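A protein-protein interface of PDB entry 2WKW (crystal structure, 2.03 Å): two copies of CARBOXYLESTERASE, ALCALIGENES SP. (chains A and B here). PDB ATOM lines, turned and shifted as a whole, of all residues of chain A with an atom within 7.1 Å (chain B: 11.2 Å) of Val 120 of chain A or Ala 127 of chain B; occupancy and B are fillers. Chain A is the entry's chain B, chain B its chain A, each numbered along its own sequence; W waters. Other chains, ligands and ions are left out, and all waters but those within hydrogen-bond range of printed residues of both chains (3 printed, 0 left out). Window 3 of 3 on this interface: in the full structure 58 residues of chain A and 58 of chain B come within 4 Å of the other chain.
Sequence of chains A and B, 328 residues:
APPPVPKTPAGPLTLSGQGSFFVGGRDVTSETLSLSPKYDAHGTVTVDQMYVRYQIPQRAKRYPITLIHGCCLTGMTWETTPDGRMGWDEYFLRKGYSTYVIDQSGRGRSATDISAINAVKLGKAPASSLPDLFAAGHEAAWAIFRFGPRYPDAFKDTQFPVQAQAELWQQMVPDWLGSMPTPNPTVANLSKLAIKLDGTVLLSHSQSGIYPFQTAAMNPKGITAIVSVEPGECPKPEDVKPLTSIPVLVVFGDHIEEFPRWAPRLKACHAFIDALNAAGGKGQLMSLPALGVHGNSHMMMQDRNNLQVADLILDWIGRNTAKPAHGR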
ATOM      1  N   THR A  32     -26.332  17.712   5.285  1.00  0.00           N
ATOM      2  CA  THR A  32     -24.988  18.062   4.820  1.00  0.00           C
ATOM      3  C   THR A  32     -24.692  19.567   4.952  1.00  0.00           C
ATOM      4  O   THR A  32     -24.004  20.128   4.099  1.00  0.00           O
ATOM      5  CB  THR A  32     -24.820  17.661   3.348  1.00  0.00           C
ATOM      6  OG1 THR A  32     -25.911  18.214   2.601  1.00  0.00           O
ATOM      7  CG2 THR A  32     -24.803  16.131   3.180  1.00  0.00           C
ATOM      8  N   ILE A 114     -26.589  24.916  -0.364  1.00  0.00           N
ATOM      9  CA  ILE A 114     -25.275  24.292  -0.606  1.00  0.00           C
ATOM     10  C   ILE A 114     -25.258  22.790  -0.223  1.00  0.00           C
ATOM     11  O   ILE A 114     -24.207  22.167  -0.192  1.00  0.00           O
ATOM     12  CB  ILE A 114     -24.103  25.079   0.086  1.00  0.00           C
ATOM     13  CG1 ILE A 114     -24.350  25.333   1.595  1.00  0.00           C
ATOM     14  CG2 ILE A 114     -23.883  26.430  -0.643  1.00  0.00           C
ATOM     15  CD1 ILE A 114     -24.306  24.083   2.523  1.00  0.00           C
ATOM     16  N   SER A 115     -26.432  22.221   0.062  1.00  0.00           N
ATOM     17  CA  SER A 115     -26.531  20.834   0.542  1.00  0.00           C
ATOM     18  C   SER A 115     -25.927  19.795  -0.392  1.00  0.00           C
ATOM     19  O   SER A 115     -25.210  18.896   0.061  1.00  0.00           O
ATOM     20  CB  SER A 115     -28.002  20.460   0.787  1.00  0.00           C
ATOM     21  OG  SER A 115     -28.449  21.077   1.969  1.00  0.00           O
ATOM     22  N   ALA A 116     -26.267  19.891  -1.675  1.00  0.00           N
ATOM     23  CA  ALA A 116     -25.780  18.945  -2.660  1.00  0.00           C
ATOM     24  C   ALA A 116     -24.260  19.033  -2.825  1.00  0.00           C
ATOM     25  O   ALA A 116     -23.601  18.004  -2.998  1.00  0.00           O
ATOM     26  CB  ALA A 116     -26.495  19.122  -3.992  1.00  0.00           C
ATOM     27  N   ILE A 117     -23.691  20.244  -2.765  1.00  0.00           N
ATOM     28  CA  ILE A 117     -22.223  20.385  -2.866  1.00  0.00           C
ATOM     29  C   ILE A 117     -21.543  19.646  -1.713  1.00  0.00           C
ATOM     30  O   ILE A 117     -20.634  18.841  -1.937  1.00  0.00           O
ATOM     31  CB  ILE A 117     -21.740  21.870  -2.936  1.00  0.00           C
ATOM     32  CG1 ILE A 117     -22.220  22.527  -4.233  1.00  0.00           C
ATOM     33  CG2 ILE A 117     -20.197  21.947  -2.923  1.00  0.00           C
ATOM     34  CD1 ILE A 117     -22.397  24.049  -4.131  1.00  0.00           C
ATOM     35  N   ASN A 118     -21.981  19.911  -0.483  1.00  0.00           N
ATOM     36  CA  ASN A 118     -21.375  19.267   0.679  1.00  0.00           C
ATOM     37  C   ASN A 118     -21.638  17.757   0.655  1.00  0.00           C
ATOM     38  O   ASN A 118     -20.790  16.978   1.078  1.00  0.00           O
ATOM     39  CB  ASN A 118     -21.887  19.873   1.990  1.00  0.00           C
ATOM     40  CG  ASN A 118     -21.234  21.211   2.325  1.00  0.00           C
ATOM     41  OD1 ASN A 118     -20.338  21.684   1.619  1.00  0.00           O
ATOM     42  ND2 ASN A 118     -21.681  21.821   3.418  1.00  0.00           N
ATOM     43  N   ALA A 119     -22.809  17.362   0.146  1.00  0.00           N
ATOM     44  CA  ALA A 119     -23.131  15.934   0.006  1.00  0.00           C
ATOM     45  C   ALA A 119     -22.093  15.228  -0.845  1.00  0.00           C
ATOM     46  O   ALA A 119     -21.630  14.136  -0.481  1.00  0.00           O
ATOM     47  CB  ALA A 119     -24.543  15.724  -0.580  1.00  0.00           C
ATOM     48  N   VAL A 120     -21.716  15.847  -1.968  1.00  0.00           N
ATOM     49  CA  VAL A 120     -20.736  15.234  -2.863  1.00  0.00           C
ATOM     50  C   VAL A 120     -19.387  15.149  -2.157  1.00  0.00           C
ATOM     51  O   VAL A 120     -18.755  14.094  -2.160  1.00  0.00           O
ATOM     52  CB  VAL A 120     -20.633  15.936  -4.224  1.00  0.00           C
ATOM     53  CG1 VAL A 120     -19.504  15.343  -5.048  1.00  0.00           C
ATOM     54  CG2 VAL A 120     -21.970  15.813  -4.979  1.00  0.00           C
ATOM     55  N   LYS A 121     -18.970  16.239  -1.522  1.00  0.00           N
ATOM     56  CA  LYS A 121     -17.707  16.258  -0.790  1.00  0.00           C
ATOM     57  C   LYS A 121     -17.670  15.234   0.361  1.00  0.00           C
ATOM     58  O   LYS A 121     -16.598  14.722   0.702  1.00  0.00           O
ATOM     59  CB  LYS A 121     -17.427  17.648  -0.243  1.00  0.00           C
ATOM     60  CG  LYS A 121     -16.012  17.798   0.263  1.00  0.00           C
ATOM     61  CD  LYS A 121     -15.636  19.245   0.489  1.00  0.00           C
ATOM     62  CE  LYS A 121     -14.161  19.317   0.785  1.00  0.00           C
ATOM     63  NZ  LYS A 121     -13.739  20.706   0.964  1.00  0.00           N
ATOM     64  N   LEU A 122     -18.834  14.953   0.952  1.00  0.00           N
ATOM     65  CA  LEU A 122     -18.954  13.974   2.049  1.00  0.00           C
ATOM     66  C   LEU A 122     -19.161  12.516   1.603  1.00  0.00           C
ATOM     67  O   LEU A 122     -19.120  11.615   2.437  1.00  0.00           O
ATOM     68  CB  LEU A 122     -20.069  14.372   3.033  1.00  0.00           C
ATOM     69  CG  LEU A 122     -19.837  15.614   3.902  1.00  0.00           C
ATOM     70  CD1 LEU A 122     -21.148  16.084   4.522  1.00  0.00           C
ATOM     71  CD2 LEU A 122     -18.751  15.406   4.983  1.00  0.00           C
ATOM     72  N   GLY A 123     -19.368  12.284   0.307  1.00  0.00           N
ATOM     73  CA  GLY A 123     -19.666  10.953  -0.200  1.00  0.00           C
ATOM     74  C   GLY A 123     -21.142  10.559  -0.097  1.00  0.00           C
ATOM     75  O   GLY A 123     -21.506   9.451  -0.475  1.00  0.00           O
ATOM     76  N   LYS A 124     -21.996  11.456   0.392  1.00  0.00           N
ATOM     77  CA  LYS A 124     -23.436  11.188   0.549  1.00  0.00           C
ATOM     78  C   LYS A 124     -24.272  11.409  -0.729  1.00  0.00           C
ATOM     79  O   LYS A 124     -25.515  11.469  -0.665  1.00  0.00           O
ATOM     80  CB  LYS A 124     -24.022  12.023   1.706  1.00  0.00           C
ATOM     81  CG  LYS A 124     -23.389  11.768   3.072  1.00  0.00           C
ATOM     82  CD  LYS A 124     -24.338  12.192   4.191  1.00  0.00           C
ATOM     83  CE  LYS A 124     -23.833  11.707   5.548  1.00  0.00           C
ATOM     84  NZ  LYS A 124     -24.827  11.912   6.651  1.00  0.00           N
ATOM     85  N   ALA A 125     -23.595  11.537  -1.875  1.00  0.00           N
ATOM     86  CA  ALA A 125     -24.242  11.794  -3.176  1.00  0.00           C
ATOM     87  C   ALA A 125     -23.219  11.752  -4.300  1.00  0.00           C
ATOM     88  O   ALA A 125     -22.064  12.076  -4.081  1.00  0.00           O
ATOM     89  CB  ALA A 125     -24.971  13.158  -3.174  1.00  0.00           C
ATOM     90  N   PRO A 126     -23.636  11.351  -5.515  1.00  0.00           N
ATOM     91  CA  PRO A 126     -22.684  11.366  -6.634  1.00  0.00           C
ATOM     92  C   PRO A 126     -22.482  12.776  -7.210  1.00  0.00           C
ATOM     93  O   PRO A 126     -23.365  13.645  -7.053  1.00  0.00           O
ATOM     94  CB  PRO A 126     -23.360  10.488  -7.685  1.00  0.00           C
ATOM     95  CG  PRO A 126     -24.818  10.553  -7.376  1.00  0.00           C
ATOM     96  CD  PRO A 126     -24.969  10.850  -5.907  1.00  0.00           C
ATOM     97  N   ALA A 127     -21.351  12.969  -7.886  1.00  0.00           N
ATOM     98  CA  ALA A 127     -20.992  14.239  -8.498  1.00  0.00           C
ATOM     99  C   ALA A 127     -22.088  14.812  -9.421  1.00  0.00           C
ATOM    100  O   ALA A 127     -22.074  16.007  -9.737  1.00  0.00           O
ATOM    101  CB  ALA A 127     -19.667  14.110  -9.244  1.00  0.00           C
ATOM    102  N   SER A 128     -23.032  13.955  -9.826  1.00  0.00           N
ATOM    103  CA  SER A 128     -24.101  14.314 -10.765  1.00  0.00           C
ATOM    104  C   SER A 128     -25.133  15.166 -10.054  1.00  0.00           C
ATOM    105  O   SER A 128     -25.848  15.953 -10.678  1.00  0.00           O
ATOM    106  CB  SER A 128     -24.774  13.041 -11.348  1.00  0.00           C
ATOM    107  OG  SER A 128     -25.725  12.452 -10.448  1.00  0.00           O
ATOM    108  N   SER A 129     -25.211  14.986  -8.738  1.00  0.00           N
ATOM    109  CA  SER A 129     -26.035  15.813  -7.886  1.00  0.00           C
ATOM    110  C   SER A 129     -25.533  17.265  -7.783  1.00  0.00           C
ATOM    111  O   SER A 129     -26.272  18.124  -7.285  1.00  0.00           O
ATOM    112  CB  SER A 129     -26.121  15.198  -6.479  1.00  0.00           C
ATOM    113  OG  SER A 129     -26.957  14.054  -6.450  1.00  0.00           O
ATOM    114  N   LEU A 130     -24.291  17.534  -8.211  1.00  0.00           N
ATOM    115  CA  LEU A 130     -23.768  18.917  -8.188  1.00  0.00           C
ATOM    116  C   LEU A 130     -24.631  19.827  -9.064  1.00  0.00           C
ATOM    117  O   LEU A 130     -25.051  19.419 -10.161  1.00  0.00           O
ATOM    118  CB  LEU A 130     -22.299  19.006  -8.619  1.00  0.00           C
ATOM    119  CG  LEU A 130     -21.269  18.443  -7.638  1.00  0.00           C
ATOM    120  CD1 LEU A 130     -19.872  18.476  -8.246  1.00  0.00           C
ATOM    121  CD2 LEU A 130     -21.285  19.185  -6.293  1.00  0.00           C
ATOM    122  N   PRO A 131     -24.902  21.058  -8.592  1.00  0.00           N
ATOM    123  CA  PRO A 131     -25.767  21.974  -9.353  1.00  0.00           C
ATOM    124  C   PRO A 131     -25.084  22.489 -10.624  1.00  0.00           C
ATOM    125  O   PRO A 131     -23.859  22.614 -10.634  1.00  0.00           O
ATOM    126  CB  PRO A 131     -25.985  23.135  -8.378  1.00  0.00           C
ATOM    127  CG  PRO A 131     -24.760  23.116  -7.473  1.00  0.00           C
ATOM    128  CD  PRO A 131     -24.400  21.660  -7.336  1.00  0.00           C
ATOM    129  N   SER B 115     -15.642  27.979 -10.017  1.00  0.00           N
ATOM    130  CA  SER B 115     -14.797  27.123 -10.883  1.00  0.00           C
ATOM    131  C   SER B 115     -14.562  25.729 -10.341  1.00  0.00           C
ATOM    132  O   SER B 115     -14.650  24.762 -11.098  1.00  0.00           O
ATOM    133  CB  SER B 115     -13.437  27.793 -11.163  1.00  0.00           C
ATOM    134  OG  SER B 115     -13.663  28.937 -11.970  1.00  0.00           O
ATOM    135  N   ALA B 116     -14.265  25.620  -9.040  1.00  0.00           N
ATOM    136  CA  ALA B 116     -13.970  24.310  -8.432  1.00  0.00           C
ATOM    137  C   ALA B 116     -15.168  23.363  -8.418  1.00  0.00           C
ATOM    138  O   ALA B 116     -15.008  22.148  -8.508  1.00  0.00           O
ATOM    139  CB  ALA B 116     -13.391  24.474  -7.017  1.00  0.00           C
ATOM    140  N   ILE B 117     -16.374  23.908  -8.287  1.00  0.00           N
ATOM    141  CA  ILE B 117     -17.573  23.065  -8.300  1.00  0.00           C
ATOM    142  C   ILE B 117     -17.756  22.478  -9.716  1.00  0.00           C
ATOM    143  O   ILE B 117     -17.986  21.268  -9.878  1.00  0.00           O
ATOM    144  CB  ILE B 117     -18.827  23.847  -7.832  1.00  0.00           C
ATOM    145  CG1 ILE B 117     -18.627  24.329  -6.388  1.00  0.00           C
ATOM    146  CG2 ILE B 117     -20.109  22.992  -7.992  1.00  0.00           C
ATOM    147  CD1 ILE B 117     -19.446  25.569  -6.029  1.00  0.00           C
ATOM    148  N   ASN B 118     -17.611  23.321 -10.736  1.00  0.00           N
ATOM    149  CA  ASN B 118     -17.768  22.849 -12.122  1.00  0.00           C
ATOM    150  C   ASN B 118     -16.704  21.828 -12.526  1.00  0.00           C
ATOM    151  O   ASN B 118     -17.000  20.863 -13.228  1.00  0.00           O
ATOM    152  CB  ASN B 118     -17.792  24.019 -13.099  1.00  0.00           C
ATOM    153  CG  ASN B 118     -19.158  24.735 -13.147  1.00  0.00           C
ATOM    154  OD1 ASN B 118     -20.119  24.314 -12.504  1.00  0.00           O
ATOM    155  ND2 ASN B 118     -19.222  25.837 -13.899  1.00  0.00           N
ATOM    156  N   ALA B 119     -15.473  22.034 -12.062  1.00  0.00           N
ATOM    157  CA  ALA B 119     -14.381  21.111 -12.360  1.00  0.00           C
ATOM    158  C   ALA B 119     -14.726  19.680 -11.900  1.00  0.00           C
ATOM    159  O   ALA B 119     -14.455  18.712 -12.617  1.00  0.00           O
ATOM    160  CB  ALA B 119     -13.066  21.616 -11.726  1.00  0.00           C
ATOM    161  N   VAL B 120     -15.355  19.548 -10.734  1.00  0.00           N
ATOM    162  CA  VAL B 120     -15.715  18.239 -10.202  1.00  0.00           C
ATOM    163  C   VAL B 120     -16.877  17.651 -11.006  1.00  0.00           C
ATOM    164  O   VAL B 120     -16.838  16.474 -11.392  1.00  0.00           O
ATOM    165  CB  VAL B 120     -16.044  18.294  -8.687  1.00  0.00           C
ATOM    166  CG1 VAL B 120     -16.537  16.924  -8.151  1.00  0.00           C
ATOM    167  CG2 VAL B 120     -14.823  18.768  -7.897  1.00  0.00           C
ATOM    168  N   LYS B 121     -17.887  18.471 -11.298  1.00  0.00           N
ATOM    169  CA  LYS B 121     -19.026  17.984 -12.086  1.00  0.00           C
ATOM    170  C   LYS B 121     -18.566  17.527 -13.479  1.00  0.00           C
ATOM    171  O   LYS B 121     -19.162  16.613 -14.058  1.00  0.00           O
ATOM    172  CB  LYS B 121     -20.154  19.027 -12.204  1.00  0.00           C
ATOM    173  CG  LYS B 121     -21.526  18.362 -12.576  1.00  0.00           C
ATOM    174  CD  LYS B 121     -22.610  19.397 -12.766  1.00  0.00           C
ATOM    175  CE  LYS B 121     -23.835  18.783 -13.411  1.00  0.00           C
ATOM    176  NZ  LYS B 121     -24.771  18.270 -12.407  1.00  0.00           N
ATOM    177  N   LEU B 122     -17.512  18.155 -14.005  1.00  0.00           N
ATOM    178  CA  LEU B 122     -16.950  17.766 -15.307  1.00  0.00           C
ATOM    179  C   LEU B 122     -16.017  16.547 -15.250  1.00  0.00           C
ATOM    180  O   LEU B 122     -15.444  16.144 -16.282  1.00  0.00           O
ATOM    181  CB  LEU B 122     -16.228  18.943 -15.957  1.00  0.00           C
ATOM    182  CG  LEU B 122     -17.068  20.118 -16.474  1.00  0.00           C
ATOM    183  CD1 LEU B 122     -16.167  21.324 -16.624  1.00  0.00           C
ATOM    184  CD2 LEU B 122     -17.778  19.792 -17.802  1.00  0.00           C
ATOM    185  N   GLY B 123     -15.866  15.969 -14.056  1.00  0.00           N
ATOM    186  CA  GLY B 123     -14.968  14.826 -13.845  1.00  0.00           C
ATOM    187  C   GLY B 123     -13.490  15.193 -13.967  1.00  0.00           C
ATOM    188  O   GLY B 123     -12.651  14.320 -14.142  1.00  0.00           O
ATOM    189  N   LYS B 124     -13.152  16.478 -13.867  1.00  0.00           N
ATOM    190  CA  LYS B 124     -11.742  16.892 -14.036  1.00  0.00           C
ATOM    191  C   LYS B 124     -10.975  16.979 -12.711  1.00  0.00           C
ATOM    192  O   LYS B 124      -9.741  16.982 -12.700  1.00  0.00           O
ATOM    193  CB  LYS B 124     -11.655  18.206 -14.804  1.00  0.00           C
ATOM    194  CG  LYS B 124     -12.161  18.091 -16.249  1.00  0.00           C
ATOM    195  CD  LYS B 124     -11.978  19.392 -16.996  1.00  0.00           C
ATOM    196  CE  LYS B 124     -12.386  19.216 -18.456  1.00  0.00           C
ATOM    197  NZ  LYS B 124     -12.116  20.440 -19.239  1.00  0.00           N
ATOM    198  N   ALA B 125     -11.713  17.023 -11.608  1.00  0.00           N
ATOM    199  CA  ALA B 125     -11.127  17.118 -10.266  1.00  0.00           C
ATOM    200  C   ALA B 125     -11.947  16.293  -9.310  1.00  0.00           C
ATOM    201  O   ALA B 125     -13.123  16.037  -9.575  1.00  0.00           O
ATOM    202  CB  ALA B 125     -11.057  18.585  -9.810  1.00  0.00           C
ATOM    203  N   PRO B 126     -11.338  15.848  -8.193  1.00  0.00           N
ATOM    204  CA  PRO B 126     -12.050  14.986  -7.260  1.00  0.00           C
ATOM    205  C   PRO B 126     -12.956  15.746  -6.288  1.00  0.00           C
ATOM    206  O   PRO B 126     -12.787  16.951  -6.093  1.00  0.00           O
ATOM    207  CB  PRO B 126     -10.916  14.323  -6.479  1.00  0.00           C
ATOM    208  CG  PRO B 126      -9.826  15.332  -6.512  1.00  0.00           C
ATOM    209  CD  PRO B 126      -9.899  15.934  -7.873  1.00  0.00           C
ATOM    210  N   ALA B 127     -13.895  15.025  -5.671  1.00  0.00           N
ATOM    211  CA  ALA B 127     -14.837  15.618  -4.718  1.00  0.00           C
ATOM    212  C   ALA B 127     -14.147  16.379  -3.569  1.00  0.00           C
ATOM    213  O   ALA B 127     -14.676  17.386  -3.079  1.00  0.00           O
ATOM    214  CB  ALA B 127     -15.772  14.545  -4.177  1.00  0.00           C
ATOM    215  N   SER B 128     -12.962  15.922  -3.155  1.00  0.00           N
ATOM    216  CA  SER B 128     -12.225  16.586  -2.072  1.00  0.00           C
ATOM    217  C   SER B 128     -11.776  18.003  -2.426  1.00  0.00           C
ATOM    218  O   SER B 128     -11.450  18.791  -1.526  1.00  0.00           O
ATOM    219  CB  SER B 128     -10.995  15.752  -1.627  1.00  0.00           C
ATOM    220  OG  SER B 128     -10.004  15.696  -2.654  1.00  0.00           O
ATOM    221  N   SER B 129     -11.748  18.331  -3.722  1.00  0.00           N
ATOM    222  CA  SER B 129     -11.331  19.665  -4.166  1.00  0.00           C
ATOM    223  C   SER B 129     -12.490  20.677  -4.100  1.00  0.00           C
ATOM    224  O   SER B 129     -12.309  21.875  -4.396  1.00  0.00           O
ATOM    225  CB  SER B 129     -10.731  19.612  -5.589  1.00  0.00           C
ATOM    226  OG  SER B 129     -11.734  19.385  -6.581  1.00  0.00           O
ATOM    227  N   LEU B 130     -13.676  20.194  -3.731  1.00  0.00           N
ATOM    228  CA  LEU B 130     -14.845  21.058  -3.599  1.00  0.00           C
ATOM    229  C   LEU B 130     -14.626  22.073  -2.472  1.00  0.00           C
ATOM    230  O   LEU B 130     -13.937  21.773  -1.478  1.00  0.00           O
ATOM    231  CB  LEU B 130     -16.142  20.245  -3.364  1.00  0.00           C
ATOM    232  CG  LEU B 130     -16.710  19.447  -4.551  1.00  0.00           C
ATOM    233  CD1 LEU B 130     -17.800  18.502  -4.047  1.00  0.00           C
ATOM    234  CD2 LEU B 130     -17.253  20.351  -5.678  1.00  0.00           C
ATOM    235  N   PRO B 131     -15.188  23.288  -2.626  1.00  0.00           N
ATOM    236  CA  PRO B 131     -14.960  24.331  -1.610  1.00  0.00           C
ATOM    237  C   PRO B 131     -15.580  23.934  -0.282  1.00  0.00           C
ATOM    238  O   PRO B 131     -16.525  23.122  -0.264  1.00  0.00           O
ATOM    239  CB  PRO B 131     -15.695  25.556  -2.181  1.00  0.00           C
ATOM    240  CG  PRO B 131     -16.676  25.020  -3.184  1.00  0.00           C
ATOM    241  CD  PRO B 131     -16.010  23.770  -3.754  1.00  0.00           C
ATOM    242  N   ASP B 132     -15.050  24.491   0.807  1.00  0.00           N
ATOM    243  CA  ASP B 132     -15.560  24.276   2.155  1.00  0.00           C
ATOM    244  C   ASP B 132     -16.716  25.282   2.388  1.00  0.00           C
ATOM    245  O   ASP B 132     -16.474  26.502   2.562  1.00  0.00           O
ATOM    246  CB  ASP B 132     -14.405  24.490   3.150  1.00  0.00           C
ATOM    247  CG  ASP B 132     -14.798  24.237   4.597  1.00  0.00           C
ATOM    248  OD1 ASP B 132     -15.803  23.550   4.846  1.00  0.00           O
ATOM    249  OD2 ASP B 132     -14.081  24.722   5.498  1.00  0.00           O
ATOM    250  N   LEU B 133     -17.950  24.780   2.381  1.00  0.00           N
ATOM    251  CA  LEU B 133     -19.145  25.613   2.471  1.00  0.00           C
ATOM    252  C   LEU B 133     -19.917  25.245   3.740  1.00  0.00           C
ATOM    253  O   LEU B 133     -19.859  24.094   4.209  1.00  0.00           O
ATOM    254  CB  LEU B 133     -20.029  25.381   1.226  1.00  0.00           C
ATOM    255  CG  LEU B 133     -19.351  25.612  -0.137  1.00  0.00           C
ATOM    256  CD1 LEU B 133     -20.307  25.361  -1.309  1.00  0.00           C
ATOM    257  CD2 LEU B 133     -18.726  26.988  -0.221  1.00  0.00           C
HETATM  258  O   HOH W   1     -21.248  22.048 -11.045  1.00  0.00           O
HETATM  259  O   HOH W   2     -18.295  21.231  -0.124  1.00  0.00           O
HETATM  260  O   HOH W   3     -14.005  14.641  -0.168  1.00  0.00           O
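The backbone carbonyl oxygen (O) of Ser 128 of chain A is in hydrogen-bond range of the side-chain amino group (NZ) of Lys 121 of chain B, 3.1 Å away. The side-chain amino group (NZ) of Lys 121 of chain B is in hydrogen-bond range of the backbone carbonyl oxygen (O) of Leu 130 of chain A (2.5 Å). O of Leu 130 of chain B sits at hydrogen-bond distance from NZ of Lys 121 of chain A. The backbone carbonyl oxygen (O) of Leu 133 of chain B sits at hydrogen-bond distance from the side-chain amide nitrogen (ND2) of Asn 118 of chain A (3.0 Å).
Water W2 bridges O of Pro 131 of chain B (2.6 Å) and OD1 of Asn 118 of chain A (2.7 Å). Water W1 bridges O of Pro 131 of chain A (2.7 Å) and OD1 of Asn 118 of chain B (2.9 Å). Water W3 bridges O of Lys 121 of chain A (2.7 Å) and N of Ser 128 of chain B (3.4 Å).
Ile 117 of chain A touches Leu 130 of chain B, and with the chains exchanged Leu 130 of chain A touches Ile 117 of chain B. Val 120 of chain A touches Ala 127 of chain B, but with the chains exchanged Ala 127 of chain A does not touch Val 120 of chain B (4.3 Å). Val 120 of chain A touches Leu 130 of chain B, and with the chains exchanged Leu 130 of chain A touches Val 120 of chain B. Lys 121 of chain A touches Ser 128 of chain B, and with the chains exchanged Ser 128 of chain A touches Lys 121 of chain B. 17 positions are printed for both chains.
ND2 of Asn 118 of chain A sits at hydrogen-bond distance from O of Thr 32 of chain A (3.0 Å).
Val 120 of chain A touches two residues of chain B. Ala 127 of chain B touches just these residues of chain A: Val 120 (3.6 Å) and Lys 121 (3.6 Å). No residue of chain B comes within 4 Å of Ala 119 of chain A. No residue of chain B comes within 4 Å of Pro 126 of chain A. No residue of chain B comes within 4 Å of Ser 129 of chain A. Of chain B, only Ile 117 (3.7 Å), Val 120 (3.7 Å) and Lys 121 (2.5 Å) come within 4 Å of Leu 130 of chain A. Printed residues of chain A within 4 Å of Ser 128 of chain B: Lys 121. Of the printed residues of chain A, Lys 121 of chain B touches Ala 127, Ser 128 and Leu 130. Printed residues of chain A within 4 Å of Pro 131 of chain B: Lys 121 (3.9 Å). Of the printed residues of chain A, Leu 130 of chain B touches Ile 117 (3.5 Å), Val 120 (3.7 Å) and Lys 121 (2.7 Å). Ala 116 of chain B touches none of the printed residues of chain A. Lys 124 of chain B touches none of the printed residues of chain A. The nearest residue of chain B that does not touch Val 120 of chain A is Val 120 of chain B (4.6 Å).
Hydrophobic or aromatic side chains of chain B within 4 Å of the printed part of chain A: Ile 117, Val 120, Ala 127, Leu 130 and Leu 133. Among the printed residues, no Asp or Glu carboxylate lies within 4 Å of a Lys or Arg side-chain nitrogen of the other chain.
Among the printed residues, pairs that only touch across the chains: Ile 114 of chain A with Leu 133 of chain B (3.8 Å), Ile 117 of chain A with Ile 117 of chain B (3.8 Å), Ile 117 of chain A with Leu 130 of chain B (3.5 Å), Ile 117 of chain A with Leu 133 of chain B (3.7 Å), Val 120 of chain A with Ala 127 of chain B (3.6 Å), Val 120 of chain A with Leu 130 of chain B (3.7 Å), Lys 121 of chain A with Ala 127 of chain B (3.6 Å), Lys 121 of chain A with Ser 128 of chain B (3.6 Å), Lys 121 of chain A with Pro 131 of chain B (3.9 Å), Ala 127 of chain A with Lys 121 of chain B (3.7 Å), Leu 130 of chain A with Ile 117 of chain B (3.7 Å) and Leu 130 of chain A with Val 120 of chain B (3.7 Å).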
